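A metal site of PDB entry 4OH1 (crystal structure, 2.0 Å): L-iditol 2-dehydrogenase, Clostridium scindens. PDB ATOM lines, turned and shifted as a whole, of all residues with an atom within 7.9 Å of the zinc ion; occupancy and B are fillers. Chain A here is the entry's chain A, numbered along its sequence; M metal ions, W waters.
N of OCS 46 is in hydrogen-bond range of OD2 of Asp 49.
OG1 of Thr 160 lies within hydrogen-bond range of O of Glu 157.
NZ of Lys 344 is in salt-bridge range of OE1 of Glu 75, at 2.6 Å.
The backbone carbonyl oxygen (O) of Glu 75 sits at hydrogen-bond distance from the backbone NH (N) of Ser 44 (2.9 Å).
OD2 of OCS 46 sits close to the side-chain hydroxyl (OG) of Ser 48 (3.4 Å).
Four residues have an atom within 4 Å of the zinc ion: OCS 46, His 74, Glu 75 and Glu 157.
The zinc ion is bound by the side-chain carboxylate (OE2) of Glu 75 (2.1 Å).
The zinc ion is bound by OE1 of Glu 157, at 2.1 Å.
The zinc ion is bound by OD2 of OCS 46 (2.3 Å).
The zinc ion is bound by water W1.
Water W2 binds the zinc ion (2.4 Å).
The zinc ion is bound by NE2 of His 74 (2.4 Å).
The zinc ion has six donor atoms within binding distance.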
ATOM      1  N   SER A  44     -18.336   0.560 -17.076  1.00  0.00           N
ATOM      2  CA  SER A  44     -17.981   1.439 -18.133  1.00  0.00           C
ATOM      3  C   SER A  44     -19.117   1.642 -19.101  1.00  0.00           C
ATOM      4  O   SER A  44     -19.999   0.813 -19.291  1.00  0.00           O
ATOM      5  CB  SER A  44     -16.803   0.875 -18.928  1.00  0.00           C
ATOM      6  OG  SER A  44     -16.393   1.932 -19.732  1.00  0.00           O
ATOM      7  N   ILE A  45     -19.071   2.807 -19.712  1.00  0.00           N
ATOM      8  CA  ILE A  45     -20.062   3.223 -20.668  1.00  0.00           C
ATOM      9  C   ILE A  45     -19.525   3.114 -22.070  1.00  0.00           C
ATOM     10  O   ILE A  45     -18.415   3.542 -22.385  1.00  0.00           O
ATOM     11  CB  ILE A  45     -20.404   4.686 -20.501  1.00  0.00           C
ATOM     12  CG1 ILE A  45     -20.692   5.020 -19.043  1.00  0.00           C
ATOM     13  CG2 ILE A  45     -21.616   4.977 -21.357  1.00  0.00           C
ATOM     14  CD1 ILE A  45     -20.896   6.476 -18.817  1.00  0.00           C
ATOM     15  N   OCS A  46     -20.394   2.682 -22.944  1.00  0.00           N
ATOM     16  CA  OCS A  46     -20.031   2.333 -24.266  1.00  0.00           C
ATOM     17  CB  OCS A  46     -20.682   0.965 -24.417  1.00  0.00           C
ATOM     18  SG  OCS A  46     -20.118   0.170 -25.862  1.00  0.00           S
ATOM     19  C   OCS A  46     -20.593   3.256 -25.357  1.00  0.00           C
ATOM     20  O   OCS A  46     -21.579   3.915 -25.138  1.00  0.00           O
ATOM     21  OD1 OCS A  46     -20.830   0.748 -26.940  1.00  0.00           O
ATOM     22  OD2 OCS A  46     -20.391  -1.226 -25.816  1.00  0.00           O
ATOM     23  OD3 OCS A  46     -18.695   0.438 -25.943  1.00  0.00           O
ATOM     24  N   GLY A  47     -20.010   3.222 -26.549  1.00  0.00           N
ATOM     25  CA  GLY A  47     -20.648   3.802 -27.778  1.00  0.00           C
ATOM     26  C   GLY A  47     -22.079   3.308 -28.125  1.00  0.00           C
ATOM     27  O   GLY A  47     -22.879   4.070 -28.611  1.00  0.00           O
ATOM     28  N   SER A  48     -22.401   2.036 -27.892  1.00  0.00           N
ATOM     29  CA  SER A  48     -23.769   1.524 -28.141  1.00  0.00           C
ATOM     30  C   SER A  48     -24.756   2.120 -27.146  1.00  0.00           C
ATOM     31  O   SER A  48     -25.869   2.454 -27.527  1.00  0.00           O
ATOM     32  CB  SER A  48     -23.808  -0.003 -28.068  1.00  0.00           C
ATOM     33  OG  SER A  48     -23.574  -0.454 -26.747  1.00  0.00           O
ATOM     34  N   ASP A  49     -24.357   2.256 -25.885  1.00  0.00           N
ATOM     35  CA  ASP A  49     -25.161   2.968 -24.876  1.00  0.00           C
ATOM     36  C   ASP A  49     -25.504   4.398 -25.381  1.00  0.00           C
ATOM     37  O   ASP A  49     -26.633   4.861 -25.197  1.00  0.00           O
ATOM     38  CB  ASP A  49     -24.438   3.042 -23.476  1.00  0.00           C
ATOM     39  CG  ASP A  49     -24.057   1.627 -22.877  1.00  0.00           C
ATOM     40  OD1 ASP A  49     -24.862   0.683 -22.934  1.00  0.00           O
ATOM     41  OD2 ASP A  49     -22.949   1.465 -22.314  1.00  0.00           O
ATOM     42  N   GLY A  73     -26.150  -1.466 -19.460  1.00  0.00           N
ATOM     43  CA  GLY A  73     -24.759  -1.520 -18.971  1.00  0.00           C
ATOM     44  C   GLY A  73     -24.302  -2.923 -19.198  1.00  0.00           C
ATOM     45  O   GLY A  73     -24.973  -3.853 -18.808  1.00  0.00           O
ATOM     46  N   HIS A  74     -23.188  -3.097 -19.892  1.00  0.00           N
ATOM     47  CA  HIS A  74     -22.669  -4.434 -20.144  1.00  0.00           C
ATOM     48  C   HIS A  74     -21.124  -4.535 -20.005  1.00  0.00           C
ATOM     49  O   HIS A  74     -20.512  -5.512 -20.458  1.00  0.00           O
ATOM     50  CB  HIS A  74     -23.132  -4.878 -21.526  1.00  0.00           C
ATOM     51  CG  HIS A  74     -22.530  -4.059 -22.598  1.00  0.00           C
ATOM     52  ND1 HIS A  74     -22.992  -2.798 -22.904  1.00  0.00           N
ATOM     53  CD2 HIS A  74     -21.449  -4.262 -23.371  1.00  0.00           C
ATOM     54  CE1 HIS A  74     -22.228  -2.264 -23.840  1.00  0.00           C
ATOM     55  NE2 HIS A  74     -21.289  -3.140 -24.146  1.00  0.00           N
ATOM     56  N   GLU A  75     -20.504  -3.535 -19.389  1.00  0.00           N
ATOM     57  CA  GLU A  75     -19.081  -3.502 -19.212  1.00  0.00           C
ATOM     58  C   GLU A  75     -18.835  -3.297 -17.735  1.00  0.00           C
ATOM     59  O   GLU A  75     -19.090  -2.205 -17.229  1.00  0.00           O
ATOM     60  CB  GLU A  75     -18.479  -2.370 -20.014  1.00  0.00           C
ATOM     61  CG  GLU A  75     -18.823  -2.411 -21.508  1.00  0.00           C
ATOM     62  CD  GLU A  75     -18.097  -1.298 -22.350  1.00  0.00           C
ATOM     63  OE1 GLU A  75     -17.423  -0.384 -21.812  1.00  0.00           O
ATOM     64  OE2 GLU A  75     -18.165  -1.384 -23.581  1.00  0.00           O
ATOM     65  N   TYR A 102     -22.227 -10.116 -20.785  1.00  0.00           N
ATOM     66  CA  TYR A 102     -23.641  -9.818 -20.846  1.00  0.00           C
ATOM     67  C   TYR A 102     -24.366 -10.889 -21.630  1.00  0.00           C
ATOM     68  O   TYR A 102     -25.566 -11.099 -21.425  1.00  0.00           O
ATOM     69  CB  TYR A 102     -23.888  -8.426 -21.505  1.00  0.00           C
ATOM     70  CG  TYR A 102     -23.460  -8.366 -22.976  1.00  0.00           C
ATOM     71  CD1 TYR A 102     -22.153  -8.043 -23.335  1.00  0.00           C
ATOM     72  CD2 TYR A 102     -24.325  -8.698 -23.978  1.00  0.00           C
ATOM     73  CE1 TYR A 102     -21.742  -8.029 -24.664  1.00  0.00           C
ATOM     74  CE2 TYR A 102     -23.923  -8.698 -25.318  1.00  0.00           C
ATOM     75  CZ  TYR A 102     -22.639  -8.351 -25.652  1.00  0.00           C
ATOM     76  OH  TYR A 102     -22.220  -8.381 -26.969  1.00  0.00           O
ATOM     77  N   ALA A 154     -12.906  -3.515 -15.781  1.00  0.00           N
ATOM     78  CA  ALA A 154     -14.183  -3.097 -16.298  1.00  0.00           C
ATOM     79  C   ALA A 154     -14.157  -2.989 -17.846  1.00  0.00           C
ATOM     80  O   ALA A 154     -15.199  -3.005 -18.493  1.00  0.00           O
ATOM     81  CB  ALA A 154     -14.553  -1.757 -15.740  1.00  0.00           C
ATOM     82  N   LEU A 155     -12.983  -2.827 -18.416  1.00  0.00           N
ATOM     83  CA  LEU A 155     -12.869  -2.727 -19.883  1.00  0.00           C
ATOM     84  C   LEU A 155     -12.655  -4.056 -20.544  1.00  0.00           C
ATOM     85  O   LEU A 155     -12.380  -4.057 -21.727  1.00  0.00           O
ATOM     86  CB  LEU A 155     -11.780  -1.737 -20.326  1.00  0.00           C
ATOM     87  CG  LEU A 155     -12.389  -0.339 -20.381  1.00  0.00           C
ATOM     88  CD1 LEU A 155     -13.091   0.101 -19.080  1.00  0.00           C
ATOM     89  CD2 LEU A 155     -11.254   0.587 -20.656  1.00  0.00           C
ATOM     90  N   VAL A 156     -12.795  -5.169 -19.832  1.00  0.00           N
ATOM     91  CA  VAL A 156     -12.646  -6.465 -20.464  1.00  0.00           C
ATOM     92  C   VAL A 156     -13.528  -6.691 -21.655  1.00  0.00           C
ATOM     93  O   VAL A 156     -13.068  -7.291 -22.688  1.00  0.00           O
ATOM     94  CB  VAL A 156     -12.779  -7.643 -19.481  1.00  0.00           C
ATOM     95  CG1 VAL A 156     -12.955  -8.960 -20.201  1.00  0.00           C
ATOM     96  CG2 VAL A 156     -11.531  -7.753 -18.611  1.00  0.00           C
ATOM     97  N   GLU A 157     -14.777  -6.246 -21.601  1.00  0.00           N
ATOM     98  CA  GLU A 157     -15.712  -6.583 -22.683  1.00  0.00           C
ATOM     99  C   GLU A 157     -15.359  -5.776 -23.936  1.00  0.00           C
ATOM    100  O   GLU A 157     -15.323  -6.318 -25.022  1.00  0.00           O
ATOM    101  CB  GLU A 157     -17.184  -6.409 -22.311  1.00  0.00           C
ATOM    102  CG  GLU A 157     -18.206  -6.806 -23.445  1.00  0.00           C
ATOM    103  CD  GLU A 157     -18.419  -5.707 -24.464  1.00  0.00           C
ATOM    104  OE1 GLU A 157     -18.142  -4.538 -24.122  1.00  0.00           O
ATOM    105  OE2 GLU A 157     -18.784  -5.992 -25.638  1.00  0.00           O
ATOM    106  N   PRO A 158     -15.138  -4.475 -23.801  1.00  0.00           N
ATOM    107  CA  PRO A 158     -14.774  -3.811 -25.044  1.00  0.00           C
ATOM    108  C   PRO A 158     -13.435  -4.289 -25.630  1.00  0.00           C
ATOM    109  O   PRO A 158     -13.309  -4.336 -26.851  1.00  0.00           O
ATOM    110  CB  PRO A 158     -14.747  -2.340 -24.682  1.00  0.00           C
ATOM    111  CG  PRO A 158     -14.741  -2.275 -23.250  1.00  0.00           C
ATOM    112  CD  PRO A 158     -15.413  -3.524 -22.746  1.00  0.00           C
ATOM    113  N   LEU A 159     -12.481  -4.689 -24.788  1.00  0.00           N
ATOM    114  CA  LEU A 159     -11.247  -5.330 -25.283  1.00  0.00           C
ATOM    115  C   LEU A 159     -11.546  -6.579 -26.078  1.00  0.00           C
ATOM    116  O   LEU A 159     -10.879  -6.811 -27.092  1.00  0.00           O
ATOM    117  CB  LEU A 159     -10.254  -5.590 -24.183  1.00  0.00           C
ATOM    118  CG  LEU A 159      -8.821  -5.943 -24.587  1.00  0.00           C
ATOM    119  CD1 LEU A 159      -8.137  -4.717 -25.321  1.00  0.00           C
ATOM    120  CD2 LEU A 159      -8.064  -6.268 -23.360  1.00  0.00           C
ATOM    121  N   THR A 160     -12.549  -7.376 -25.695  1.00  0.00           N
ATOM    122  CA  THR A 160     -12.909  -8.496 -26.548  1.00  0.00           C
ATOM    123  C   THR A 160     -13.348  -8.098 -27.960  1.00  0.00           C
ATOM    124  O   THR A 160     -13.174  -8.857 -28.905  1.00  0.00           O
ATOM    125  CB  THR A 160     -14.031  -9.382 -25.976  1.00  0.00           C
ATOM    126  OG1 THR A 160     -15.266  -8.649 -25.935  1.00  0.00           O
ATOM    127  CG2 THR A 160     -13.680  -9.925 -24.564  1.00  0.00           C
ATOM    128  N   VAL A 161     -14.076  -6.992 -28.075  1.00  0.00           N
ATOM    129  CA  VAL A 161     -14.478  -6.498 -29.350  1.00  0.00           C
ATOM    130  C   VAL A 161     -13.265  -6.019 -30.167  1.00  0.00           C
ATOM    131  O   VAL A 161     -13.128  -6.285 -31.339  1.00  0.00           O
ATOM    132  CB  VAL A 161     -15.474  -5.326 -29.190  1.00  0.00           C
ATOM    133  CG1 VAL A 161     -15.774  -4.721 -30.541  1.00  0.00           C
ATOM    134  CG2 VAL A 161     -16.781  -5.813 -28.573  1.00  0.00           C
ATOM    135  N   LEU A 185     -12.469   2.321 -28.359  1.00  0.00           N
ATOM    136  CA  LEU A 185     -12.132   1.116 -29.130  1.00  0.00           C
ATOM    137  C   LEU A 185     -10.937   1.362 -30.053  1.00  0.00           C
ATOM    138  O   LEU A 185     -10.079   0.504 -30.209  1.00  0.00           O
ATOM    139  CB  LEU A 185     -13.301   0.638 -29.975  1.00  0.00           C
ATOM    140  CG  LEU A 185     -14.356  -0.165 -29.255  1.00  0.00           C
ATOM    141  CD1 LEU A 185     -15.395  -0.696 -30.280  1.00  0.00           C
ATOM    142  CD2 LEU A 185     -13.758  -1.314 -28.412  1.00  0.00           C
ATOM    143  N   MET A 188      -7.784   1.222 -28.011  1.00  0.00           N
ATOM    144  CA  MET A 188      -7.437  -0.180 -27.759  1.00  0.00           C
ATOM    145  C   MET A 188      -6.866  -0.888 -29.014  1.00  0.00           C
ATOM    146  O   MET A 188      -5.970  -1.693 -28.889  1.00  0.00           O
ATOM    147  CB  MET A 188      -8.659  -0.973 -27.276  1.00  0.00           C
ATOM    148  CG  MET A 188      -9.199  -0.417 -25.981  1.00  0.00           C
ATOM    149  SD  MET A 188     -10.731  -1.429 -25.210  1.00  0.00           S
ATOM    150  CE  MET A 188     -11.781   0.201 -24.772  1.00  0.00           C
ATOM    151  N   LYS A 344     -12.990   6.776 -22.913  1.00  0.00           N
ATOM    152  CA  LYS A 344     -13.818   5.896 -22.065  1.00  0.00           C
ATOM    153  C   LYS A 344     -14.038   6.569 -20.709  1.00  0.00           C
ATOM    154  O   LYS A 344     -13.124   7.203 -20.140  1.00  0.00           O
ATOM    155  CB  LYS A 344     -13.165   4.515 -21.798  1.00  0.00           C
ATOM    156  CG  LYS A 344     -13.208   3.521 -22.938  1.00  0.00           C
ATOM    157  CD  LYS A 344     -14.602   3.144 -23.407  1.00  0.00           C
ATOM    158  CE  LYS A 344     -15.120   1.920 -22.737  1.00  0.00           C
ATOM    159  NZ  LYS A 344     -16.387   1.469 -23.393  1.00  0.00           N
HETATM  160 ZN    ZN M   1     -18.991  -2.774 -24.869  1.00  0.00          ZN
HETATM  161  O   HOH W   1     -19.888  -4.049 -26.672  1.00  0.00           O
HETATM  162  O   HOH W   2     -17.615  -2.318 -26.771  1.00  0.00           O
